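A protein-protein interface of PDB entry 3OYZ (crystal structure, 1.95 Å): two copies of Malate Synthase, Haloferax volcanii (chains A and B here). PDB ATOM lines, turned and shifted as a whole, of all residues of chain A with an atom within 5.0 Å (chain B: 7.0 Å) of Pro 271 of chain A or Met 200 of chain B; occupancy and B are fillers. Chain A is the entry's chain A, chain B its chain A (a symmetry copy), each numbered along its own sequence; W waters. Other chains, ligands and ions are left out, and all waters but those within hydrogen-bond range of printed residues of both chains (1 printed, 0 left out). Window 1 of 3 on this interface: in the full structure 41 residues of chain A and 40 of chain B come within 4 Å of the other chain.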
ATOM      1  N   ARG A  12       0.248   2.383  -8.105  1.00  0.00           N
ATOM      2  CA  ARG A  12      -0.236   1.099  -8.599  1.00  0.00           C
ATOM      3  C   ARG A  12      -0.303   0.078  -7.504  1.00  0.00           C
ATOM      4  O   ARG A  12      -1.178  -0.791  -7.556  1.00  0.00           O
ATOM      5  CB  ARG A  12       0.748   0.532  -9.674  1.00  0.00           C
ATOM      6  CG  ARG A  12       0.794   1.385 -10.947  1.00  0.00           C
ATOM      7  CD  ARG A  12       1.956   0.912 -11.859  1.00  0.00           C
ATOM      8  NE  ARG A  12       3.201   1.296 -11.198  1.00  0.00           N
ATOM      9  CZ  ARG A  12       4.408   0.949 -11.662  1.00  0.00           C
ATOM     10  NH1 ARG A  12       4.501   0.200 -12.761  1.00  0.00           N
ATOM     11  NH2 ARG A  12       5.491   1.429 -11.067  1.00  0.00           N
ATOM     12  N   THR A 246      -8.756  -4.935 -13.272  1.00  0.00           N
ATOM     13  CA  THR A 246      -9.447  -4.388 -14.429  1.00  0.00           C
ATOM     14  C   THR A 246     -10.784  -3.789 -14.019  1.00  0.00           C
ATOM     15  O   THR A 246     -11.093  -2.706 -14.493  1.00  0.00           O
ATOM     16  CB  THR A 246      -9.693  -5.468 -15.484  1.00  0.00           C
ATOM     17  OG1 THR A 246      -8.417  -5.922 -15.942  1.00  0.00           O
ATOM     18  CG2 THR A 246     -10.474  -4.879 -16.621  1.00  0.00           C
ATOM     19  N   GLN A 249     -10.013  -0.427 -12.280  1.00  0.00           N
ATOM     20  CA  GLN A 249      -9.505   0.603 -13.179  1.00  0.00           C
ATOM     21  C   GLN A 249     -10.724   1.216 -13.885  1.00  0.00           C
ATOM     22  O   GLN A 249     -10.704   2.401 -14.246  1.00  0.00           O
ATOM     23  CB  GLN A 249      -8.490  -0.022 -14.173  1.00  0.00           C
ATOM     24  CG  GLN A 249      -7.132  -0.379 -13.473  1.00  0.00           C
ATOM     25  CD  GLN A 249      -6.345  -1.511 -14.188  1.00  0.00           C
ATOM     26  OE1 GLN A 249      -6.646  -1.847 -15.330  1.00  0.00           O
ATOM     27  NE2 GLN A 249      -5.364  -2.074 -13.524  1.00  0.00           N
ATOM     28  N   ALA A 250     -11.765   0.443 -14.110  1.00  0.00           N
ATOM     29  CA  ALA A 250     -12.948   1.037 -14.779  1.00  0.00           C
ATOM     30  C   ALA A 250     -13.772   1.945 -13.848  1.00  0.00           C
ATOM     31  O   ALA A 250     -14.651   2.664 -14.334  1.00  0.00           O
ATOM     32  CB  ALA A 250     -13.853  -0.016 -15.389  1.00  0.00           C
ATOM     33  N   LEU A 254      -6.984   3.049  -9.462  1.00  0.00           N
ATOM     34  CA  LEU A 254      -5.928   2.490 -10.338  1.00  0.00           C
ATOM     35  C   LEU A 254      -4.868   1.797  -9.513  1.00  0.00           C
ATOM     36  O   LEU A 254      -3.925   1.238 -10.078  1.00  0.00           O
ATOM     37  CB  LEU A 254      -5.301   3.606 -11.183  1.00  0.00           C
ATOM     38  CG  LEU A 254      -6.243   4.440 -12.055  1.00  0.00           C
ATOM     39  CD1 LEU A 254      -5.541   5.526 -12.904  1.00  0.00           C
ATOM     40  CD2 LEU A 254      -7.210   3.620 -12.951  1.00  0.00           C
ATOM     41  N   ALA A 267       0.430  -6.424 -10.078  1.00  0.00           N
ATOM     42  CA  ALA A 267      -0.295  -5.167  -9.938  1.00  0.00           C
ATOM     43  C   ALA A 267       0.535  -4.033 -10.521  1.00  0.00           C
ATOM     44  O   ALA A 267      -0.020  -3.034 -10.951  1.00  0.00           O
ATOM     45  CB  ALA A 267      -0.629  -4.906  -8.433  1.00  0.00           C
ATOM     46  N   ASN A 268       1.857  -4.145 -10.590  1.00  0.00           N
ATOM     47  CA  ASN A 268       2.679  -3.117 -11.287  1.00  0.00           C
ATOM     48  C   ASN A 268       2.514  -3.087 -12.797  1.00  0.00           C
ATOM     49  O   ASN A 268       2.653  -2.036 -13.458  1.00  0.00           O
ATOM     50  CB  ASN A 268       4.175  -3.249 -10.958  1.00  0.00           C
ATOM     51  CG  ASN A 268       4.593  -2.462  -9.744  1.00  0.00           C
ATOM     52  OD1 ASN A 268       3.983  -1.431  -9.411  1.00  0.00           O
ATOM     53  ND2 ASN A 268       5.611  -2.966  -9.033  1.00  0.00           N
ATOM     54  N   THR A 269       2.155  -4.231 -13.351  1.00  0.00           N
ATOM     55  CA  THR A 269       2.046  -4.375 -14.808  1.00  0.00           C
ATOM     56  C   THR A 269       0.638  -4.165 -15.311  1.00  0.00           C
ATOM     57  O   THR A 269       0.417  -3.628 -16.392  1.00  0.00           O
ATOM     58  CB  THR A 269       2.332  -5.864 -15.250  1.00  0.00           C
ATOM     59  OG1 THR A 269       3.383  -6.418 -14.456  1.00  0.00           O
ATOM     60  CG2 THR A 269       2.711  -5.930 -16.689  1.00  0.00           C
ATOM     61  N   SER A 270      -0.334  -4.614 -14.531  1.00  0.00           N
ATOM     62  CA  SER A 270      -1.716  -4.558 -14.977  1.00  0.00           C
ATOM     63  C   SER A 270      -2.222  -3.217 -15.527  1.00  0.00           C
ATOM     64  O   SER A 270      -2.877  -3.255 -16.556  1.00  0.00           O
ATOM     65  CB  SER A 270      -2.680  -5.035 -13.892  1.00  0.00           C
ATOM     66  OG  SER A 270      -3.968  -4.517 -14.233  1.00  0.00           O
ATOM     67  N   PRO A 271      -1.944  -2.053 -14.900  1.00  0.00           N
ATOM     68  CA  PRO A 271      -2.592  -0.895 -15.516  1.00  0.00           C
ATOM     69  C   PRO A 271      -1.801  -0.211 -16.631  1.00  0.00           C
ATOM     70  O   PRO A 271      -2.282   0.763 -17.209  1.00  0.00           O
ATOM     71  CB  PRO A 271      -2.682   0.094 -14.341  1.00  0.00           C
ATOM     72  CG  PRO A 271      -1.472  -0.234 -13.492  1.00  0.00           C
ATOM     73  CD  PRO A 271      -1.503  -1.738 -13.525  1.00  0.00           C
ATOM     74  N   LEU A 272      -0.588  -0.698 -16.888  1.00  0.00           N
ATOM     75  CA  LEU A 272       0.235  -0.308 -18.025  1.00  0.00           C
ATOM     76  C   LEU A 272      -0.442  -0.716 -19.333  1.00  0.00           C
ATOM     77  O   LEU A 272      -0.950  -1.820 -19.479  1.00  0.00           O
ATOM     78  CB  LEU A 272       1.649  -0.877 -17.865  1.00  0.00           C
ATOM     79  CG  LEU A 272       2.408  -0.419 -16.610  1.00  0.00           C
ATOM     80  CD1 LEU A 272       3.795  -0.999 -16.603  1.00  0.00           C
ATOM     81  CD2 LEU A 272       2.502   1.086 -16.387  1.00  0.00           C
ATOM     82  N   PRO A 273      -0.521   0.198 -20.298  1.00  0.00           N
ATOM     83  CA  PRO A 273      -1.164  -0.245 -21.532  1.00  0.00           C
ATOM     84  C   PRO A 273      -0.364  -1.335 -22.285  1.00  0.00           C
ATOM     85  O   PRO A 273       0.824  -1.511 -22.045  1.00  0.00           O
ATOM     86  CB  PRO A 273      -1.325   1.053 -22.330  1.00  0.00           C
ATOM     87  CG  PRO A 273      -0.372   2.046 -21.732  1.00  0.00           C
ATOM     88  CD  PRO A 273      -0.006   1.581 -20.354  1.00  0.00           C
ATOM     89  N   THR B 194     -15.308  10.245 -16.729  1.00  0.00           N
ATOM     90  CA  THR B 194     -14.254   9.217 -16.834  1.00  0.00           C
ATOM     91  C   THR B 194     -12.881   9.775 -16.652  1.00  0.00           C
ATOM     92  O   THR B 194     -12.060   9.180 -15.925  1.00  0.00           O
ATOM     93  CB  THR B 194     -14.297   8.531 -18.215  1.00  0.00           C
ATOM     94  OG1 THR B 194     -15.528   7.828 -18.238  1.00  0.00           O
ATOM     95  CG2 THR B 194     -13.141   7.461 -18.431  1.00  0.00           C
ATOM     96  N   MET B 197     -12.455  11.032 -12.966  1.00  0.00           N
ATOM     97  CA  MET B 197     -12.317   9.881 -12.095  1.00  0.00           C
ATOM     98  C   MET B 197     -11.021   9.104 -12.413  1.00  0.00           C
ATOM     99  O   MET B 197     -10.638   8.230 -11.584  1.00  0.00           O
ATOM    100  CB  MET B 197     -13.568   8.960 -12.191  1.00  0.00           C
ATOM    101  CG  MET B 197     -14.923   9.701 -11.740  1.00  0.00           C
ATOM    102  SD  MET B 197     -14.849   9.720  -9.875  1.00  0.00           S
ATOM    103  CE  MET B 197     -15.481   8.057  -9.590  1.00  0.00           C
ATOM    104  N   ARG B 198     -10.348   9.423 -13.534  1.00  0.00           N
ATOM    105  CA  ARG B 198      -9.112   8.692 -13.935  1.00  0.00           C
ATOM    106  C   ARG B 198      -9.389   7.219 -14.268  1.00  0.00           C
ATOM    107  O   ARG B 198      -8.565   6.351 -14.025  1.00  0.00           O
ATOM    108  CB  ARG B 198      -7.891   8.838 -12.997  1.00  0.00           C
ATOM    109  CG  ARG B 198      -7.623  10.320 -12.685  1.00  0.00           C
ATOM    110  CD  ARG B 198      -6.313  10.693 -12.022  1.00  0.00           C
ATOM    111  NE  ARG B 198      -6.038   9.872 -10.859  1.00  0.00           N
ATOM    112  CZ  ARG B 198      -4.837   9.840 -10.282  1.00  0.00           C
ATOM    113  NH1 ARG B 198      -3.839  10.578 -10.783  1.00  0.00           N
ATOM    114  NH2 ARG B 198      -4.634   9.057  -9.235  1.00  0.00           N
ATOM    115  N   ALA B 199     -10.529   6.928 -14.884  1.00  0.00           N
ATOM    116  CA  ALA B 199     -10.839   5.556 -15.090  1.00  0.00           C
ATOM    117  C   ALA B 199     -10.176   5.123 -16.413  1.00  0.00           C
ATOM    118  O   ALA B 199      -9.914   5.937 -17.289  1.00  0.00           O
ATOM    119  CB  ALA B 199     -12.341   5.350 -15.142  1.00  0.00           C
ATOM    120  N   MET B 200     -10.035   3.819 -16.578  1.00  0.00           N
ATOM    121  CA  MET B 200      -9.575   3.302 -17.862  1.00  0.00           C
ATOM    122  C   MET B 200     -10.172   1.944 -18.130  1.00  0.00           C
ATOM    123  O   MET B 200     -10.623   1.212 -17.236  1.00  0.00           O
ATOM    124  CB  MET B 200      -8.050   3.379 -17.982  1.00  0.00           C
ATOM    125  CG  MET B 200      -7.248   2.512 -17.052  1.00  0.00           C
ATOM    126  SD  MET B 200      -5.523   3.117 -17.057  1.00  0.00           S
ATOM    127  CE  MET B 200      -4.937   1.878 -15.964  1.00  0.00           C
ATOM    128  N   THR B 201     -10.296   1.631 -19.413  1.00  0.00           N
ATOM    129  CA  THR B 201     -10.777   0.278 -19.745  1.00  0.00           C
ATOM    130  C   THR B 201      -9.874  -0.347 -20.820  1.00  0.00           C
ATOM    131  O   THR B 201      -9.313   0.419 -21.598  1.00  0.00           O
ATOM    132  CB  THR B 201     -12.207   0.367 -20.353  1.00  0.00           C
ATOM    133  OG1 THR B 201     -12.145   1.195 -21.524  1.00  0.00           O
ATOM    134  CG2 THR B 201     -13.290   0.948 -19.361  1.00  0.00           C
ATOM    135  N   PRO B 202      -9.812  -1.687 -20.941  1.00  0.00           N
ATOM    136  CA  PRO B 202      -8.943  -2.317 -21.974  1.00  0.00           C
ATOM    137  C   PRO B 202      -9.250  -1.842 -23.422  1.00  0.00           C
ATOM    138  O   PRO B 202      -8.318  -1.574 -24.186  1.00  0.00           O
ATOM    139  CB  PRO B 202      -9.250  -3.803 -21.794  1.00  0.00           C
ATOM    140  CG  PRO B 202      -9.742  -3.919 -20.360  1.00  0.00           C
ATOM    141  CD  PRO B 202     -10.663  -2.709 -20.302  1.00  0.00           C
ATOM    142  N   THR B 203     -10.511  -1.665 -23.795  1.00  0.00           N
ATOM    143  CA  THR B 203     -10.868  -1.112 -25.109  1.00  0.00           C
ATOM    144  C   THR B 203     -10.820   0.430 -25.255  1.00  0.00           C
ATOM    145  O   THR B 203     -10.769   0.944 -26.369  1.00  0.00           O
ATOM    146  CB  THR B 203     -12.252  -1.668 -25.563  1.00  0.00           C
ATOM    147  OG1 THR B 203     -13.310  -1.095 -24.769  1.00  0.00           O
ATOM    148  CG2 THR B 203     -12.332  -3.192 -25.373  1.00  0.00           C
ATOM    149  N   GLY B 204     -10.894   1.209 -24.170  1.00  0.00           N
ATOM    150  CA  GLY B 204     -10.950   2.655 -24.346  1.00  0.00           C
ATOM    151  C   GLY B 204     -12.392   3.072 -24.382  1.00  0.00           C
ATOM    152  O   GLY B 204     -12.651   4.248 -24.294  1.00  0.00           O
ATOM    153  N   GLU B 205     -13.347   2.153 -24.419  1.00  0.00           N
ATOM    154  CA  GLU B 205     -14.764   2.532 -24.365  1.00  0.00           C
ATOM    155  C   GLU B 205     -15.097   3.053 -22.926  1.00  0.00           C
ATOM    156  O   GLU B 205     -14.384   2.715 -21.954  1.00  0.00           O
ATOM    157  CB  GLU B 205     -15.684   1.342 -24.664  1.00  0.00           C
ATOM    158  CG  GLU B 205     -15.733   0.825 -26.136  1.00  0.00           C
ATOM    159  CD  GLU B 205     -15.786   1.882 -27.277  1.00  0.00           C
ATOM    160  OE1 GLU B 205     -16.739   2.690 -27.401  1.00  0.00           O
ATOM    161  OE2 GLU B 205     -14.852   1.899 -28.118  1.00  0.00           O
ATOM    162  N   PRO B 207     -16.505   3.361 -19.284  1.00  0.00           N
ATOM    163  CA  PRO B 207     -17.147   2.523 -18.280  1.00  0.00           C
ATOM    164  C   PRO B 207     -18.676   2.826 -18.207  1.00  0.00           C
ATOM    165  O   PRO B 207     -19.168   3.886 -18.567  1.00  0.00           O
ATOM    166  CB  PRO B 207     -16.509   3.001 -16.939  1.00  0.00           C
ATOM    167  CG  PRO B 207     -15.352   3.803 -17.316  1.00  0.00           C
ATOM    168  CD  PRO B 207     -15.562   4.344 -18.734  1.00  0.00           C
ATOM    169  N   TRP B 209     -20.529   3.190 -15.342  1.00  0.00           N
ATOM    170  CA  TRP B 209     -20.825   4.043 -14.135  1.00  0.00           C
ATOM    171  C   TRP B 209     -22.258   3.925 -13.624  1.00  0.00           C
ATOM    172  O   TRP B 209     -22.978   4.925 -13.500  1.00  0.00           O
ATOM    173  CB  TRP B 209     -20.586   5.504 -14.525  1.00  0.00           C
ATOM    174  CG  TRP B 209     -19.194   5.813 -14.955  1.00  0.00           C
ATOM    175  CD1 TRP B 209     -18.764   6.279 -16.161  1.00  0.00           C
ATOM    176  CD2 TRP B 209     -18.057   5.786 -14.082  1.00  0.00           C
ATOM    177  NE1 TRP B 209     -17.427   6.527 -16.086  1.00  0.00           N
ATOM    178  CE2 TRP B 209     -16.962   6.242 -14.821  1.00  0.00           C
ATOM    179  CE3 TRP B 209     -17.892   5.463 -12.725  1.00  0.00           C
ATOM    180  CZ2 TRP B 209     -15.665   6.326 -14.271  1.00  0.00           C
ATOM    181  CZ3 TRP B 209     -16.616   5.595 -12.157  1.00  0.00           C
ATOM    182  CH2 TRP B 209     -15.513   5.998 -12.946  1.00  0.00           C
ATOM    183  N   ALA B 394     -10.072  11.956 -21.807  1.00  0.00           N
ATOM    184  CA  ALA B 394     -10.238  10.628 -21.181  1.00  0.00           C
ATOM    185  C   ALA B 394      -9.285   9.551 -21.646  1.00  0.00           C
ATOM    186  O   ALA B 394      -8.866   8.695 -20.850  1.00  0.00           O
ATOM    187  CB  ALA B 394     -11.695  10.097 -21.289  1.00  0.00           C
ATOM    188  N   THR B 397      -5.461   8.980 -19.968  1.00  0.00           N
ATOM    189  CA  THR B 397      -5.102   8.384 -18.659  1.00  0.00           C
ATOM    190  C   THR B 397      -4.052   7.289 -18.648  1.00  0.00           C
ATOM    191  O   THR B 397      -3.119   7.375 -17.863  1.00  0.00           O
ATOM    192  CB  THR B 397      -6.364   7.964 -17.856  1.00  0.00           C
ATOM    193  OG1 THR B 397      -7.084   9.180 -17.665  1.00  0.00           O
ATOM    194  CG2 THR B 397      -6.007   7.339 -16.510  1.00  0.00           C
ATOM    195  N   PRO B 398      -4.172   6.264 -19.510  1.00  0.00           N
ATOM    196  CA  PRO B 398      -3.124   5.235 -19.508  1.00  0.00           C
ATOM    197  C   PRO B 398      -1.733   5.792 -19.841  1.00  0.00           C
ATOM    198  O   PRO B 398      -0.759   5.317 -19.267  1.00  0.00           O
ATOM    199  CB  PRO B 398      -3.606   4.195 -20.521  1.00  0.00           C
ATOM    200  CG  PRO B 398      -4.824   4.740 -21.171  1.00  0.00           C
ATOM    201  CD  PRO B 398      -5.293   5.975 -20.431  1.00  0.00           C
ATOM    202  N   ILE B 399      -1.663   6.864 -20.635  1.00  0.00           N
ATOM    203  CA  ILE B 399      -0.419   7.582 -20.896  1.00  0.00           C
ATOM    204  C   ILE B 399       0.085   8.402 -19.696  1.00  0.00           C
ATOM    205  O   ILE B 399       1.281   8.334 -19.399  1.00  0.00           O
ATOM    206  CB  ILE B 399      -0.545   8.577 -22.090  1.00  0.00           C
ATOM    207  CG1 ILE B 399      -1.001   7.863 -23.363  1.00  0.00           C
ATOM    208  CG2 ILE B 399       0.780   9.359 -22.305  1.00  0.00           C
ATOM    209  CD1 ILE B 399      -0.452   6.459 -23.513  1.00  0.00           C
ATOM    210  N   LEU B 401      -0.484   7.838 -16.627  1.00  0.00           N
ATOM    211  CA  LEU B 401       0.004   6.897 -15.668  1.00  0.00           C
ATOM    212  C   LEU B 401       1.393   6.406 -16.095  1.00  0.00           C
ATOM    213  O   LEU B 401       2.272   6.305 -15.256  1.00  0.00           O
ATOM    214  CB  LEU B 401      -0.953   5.715 -15.560  1.00  0.00           C
ATOM    215  CG  LEU B 401      -0.222   4.566 -14.914  1.00  0.00           C
ATOM    216  CD1 LEU B 401      -0.193   4.667 -13.440  1.00  0.00           C
ATOM    217  CD2 LEU B 401      -0.832   3.240 -15.258  1.00  0.00           C
ATOM    218  N   PHE B 402       1.556   6.034 -17.355  1.00  0.00           N
ATOM    219  CA  PHE B 402       2.874   5.576 -17.807  1.00  0.00           C
ATOM    220  C   PHE B 402       3.914   6.659 -17.500  1.00  0.00           C
ATOM    221  O   PHE B 402       4.932   6.408 -16.868  1.00  0.00           O
ATOM    222  CB  PHE B 402       2.883   5.259 -19.317  1.00  0.00           C
ATOM    223  CG  PHE B 402       4.278   4.976 -19.825  1.00  0.00           C
ATOM    224  CD1 PHE B 402       4.824   3.713 -19.681  1.00  0.00           C
ATOM    225  CD2 PHE B 402       5.087   6.002 -20.309  1.00  0.00           C
ATOM    226  CE1 PHE B 402       6.137   3.433 -20.091  1.00  0.00           C
ATOM    227  CE2 PHE B 402       6.409   5.741 -20.734  1.00  0.00           C
ATOM    228  CZ  PHE B 402       6.941   4.479 -20.588  1.00  0.00           C
ATOM    229  N   VAL B 405       4.904   6.971 -13.835  1.00  0.00           N
ATOM    230  CA  VAL B 405       5.690   5.810 -13.485  1.00  0.00           C
ATOM    231  C   VAL B 405       7.132   5.933 -14.009  1.00  0.00           C
ATOM    232  O   VAL B 405       8.086   5.725 -13.281  1.00  0.00           O
ATOM    233  CB  VAL B 405       5.074   4.540 -14.084  1.00  0.00           C
ATOM    234  CG1 VAL B 405       6.119   3.425 -14.013  1.00  0.00           C
ATOM    235  CG2 VAL B 405       3.825   4.091 -13.322  1.00  0.00           C
ATOM    236  N   ARG B 419       9.733  -3.978 -22.250  1.00  0.00           N
ATOM    237  CA  ARG B 419       8.309  -4.196 -22.522  1.00  0.00           C
ATOM    238  C   ARG B 419       7.795  -3.407 -23.734  1.00  0.00           C
ATOM    239  O   ARG B 419       7.040  -3.975 -24.522  1.00  0.00           O
ATOM    240  CB  ARG B 419       7.452  -4.092 -21.232  1.00  0.00           C
ATOM    241  CG  ARG B 419       6.144  -3.317 -21.342  1.00  0.00           C
ATOM    242  CD  ARG B 419       5.387  -3.123 -19.991  1.00  0.00           C
ATOM    243  NE  ARG B 419       3.958  -3.023 -20.292  1.00  0.00           N
ATOM    244  CZ  ARG B 419       3.107  -4.046 -20.204  1.00  0.00           C
ATOM    245  NH1 ARG B 419       3.547  -5.223 -19.783  1.00  0.00           N
ATOM    246  NH2 ARG B 419       1.826  -3.907 -20.538  1.00  0.00           N
ATOM    247  N   TYR B 420       8.216  -2.156 -23.928  1.00  0.00           N
ATOM    248  CA  TYR B 420       7.741  -1.349 -25.051  1.00  0.00           C
ATOM    249  C   TYR B 420       8.662  -1.115 -26.258  1.00  0.00           C
ATOM    250  O   TYR B 420       8.168  -0.834 -27.358  1.00  0.00           O
ATOM    251  CB  TYR B 420       7.270   0.041 -24.601  1.00  0.00           C
ATOM    252  CG  TYR B 420       6.093  -0.010 -23.652  1.00  0.00           C
ATOM    253  CD1 TYR B 420       4.824  -0.377 -24.094  1.00  0.00           C
ATOM    254  CD2 TYR B 420       6.270   0.254 -22.301  1.00  0.00           C
ATOM    255  CE1 TYR B 420       3.742  -0.458 -23.204  1.00  0.00           C
ATOM    256  CE2 TYR B 420       5.211   0.172 -21.409  1.00  0.00           C
ATOM    257  CZ  TYR B 420       3.956  -0.165 -21.868  1.00  0.00           C
ATOM    258  OH  TYR B 420       2.941  -0.218 -20.957  1.00  0.00           O
HETATM  259  O   HOH W   1     -10.856  -1.499 -16.909  1.00  0.00           O
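Hydrophobic or aromatic side chains of chain B that line the printed part of chain A: Ala 199, Met 200, Pro 202, Pro 207, Trp 209, Leu 401, Val 405 and Tyr 420.
Of the 12 printed residues of chain A, 9 touch a printed residue of chain B.
Hydrophobic or aromatic side chains of chain A within 4 Å of the printed part of chain B: Ala 250, Leu 254, Pro 271, Leu 272 and Pro 273.
Among the printed residues, no Asp or Glu carboxylate lies within 4 Å of a Lys or Arg side-chain nitrogen of the other chain.
Pro 271 of chain A touches just these residues of chain B: Met 200 and Leu 401.
Of the printed residues of chain A, Arg 419 of chain B touches Thr 269, Leu 272 and Pro 273.
Of the printed residues of chain A, Val 405 of chain B touches Arg 12.
Of the printed residues of chain A, Pro 202 of chain B touches Thr 246 (3.9 Å).
Printed residues of chain B within 4 Å of Arg 12 of chain A: Val 405.
The nearest residue of chain B that does not touch Pro 271 of chain A is Pro 398 of chain B (4.9 Å).
The nearest residue of chain A that does not touch Met 200 of chain B is Leu 254 of chain A (4.2 Å).
The nearest printed residue of chain B that does not touch Leu 254 of chain A is Thr 397 of chain B (4.1 Å).
The guanidinium group (NH1) of Arg 12 of chain A lies within hydrogen-bond range of the backbone carbonyl oxygen (O) of Asn 268 of chain A, at 3.0 Å.
NE2 of Gln 249 of chain A is in hydrogen-bond range of OG of Ser 270 of chain A (2.9 Å).
N of Ala 199 of chain B is in hydrogen-bond range of O of Thr 194 of chain B, at 2.9 Å.
The side-chain hydroxyl of Thr 194 of chain B sits at hydrogen-bond distance from the indole nitrogen of Trp 209 of chain B, 3.2 Å away.
The guanidinium group of Arg 419 of chain B is in hydrogen-bond range of the side-chain hydroxyl of Tyr 420 of chain B.
Among the printed residues, merely in contact across the chains: Arg 12 of chain A with Val 405 of chain B (3.6 Å), Thr 246 of chain A with Pro 202 of chain B (3.9 Å), Gln 249 of chain A with Ala 199 of chain B (3.3 Å), Ala 250 of chain A with Ala 199 of chain B (3.6 Å), Ala 250 of chain A with Pro 207 of chain B (3.2 Å), Ala 250 of chain A with Trp 209 of chain B (3.7 Å), Leu 254 of chain A with Arg 198 of chain B (3.2 Å), Thr 269 of chain A with Arg 419 of chain B (3.3 Å), Pro 271 of chain A with Met 200 of chain B (3.1 Å), Pro 271 of chain A with Leu 401 of chain B (3.5 Å), Leu 272 of chain A with Arg 419 of chain B (3.6 Å), Leu 272 of chain A with Tyr 420 of chain B (3.4 Å) and Pro 273 of chain A with Pro 398 of chain B (3.96 Å).
No position is printed for both chains.
Of the 17 pairs that touch across the chains among the printed residues, none has its exchanged pair printed and touching as well.
O of Gln 249 of chain A lies within hydrogen-bond range of N of Met 200 of chain B.
O of Met 200 of chain B sits close to N of Ala 250 of chain A (3.4 Å).
O of Pro 273 of chain A lies within hydrogen-bond range of NH2 of Arg 419 of chain B, 3.0 Å away.
The side-chain hydroxyl of Tyr 420 of chain B lies within hydrogen-bond range of the backbone carbonyl oxygen of Pro 273 of chain A (2.7 Å).
Water W1 lies within hydrogen-bond range of O of Thr 246 of chain A (2.7 Å) and O of Met 200 of chain B (2.7 Å).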
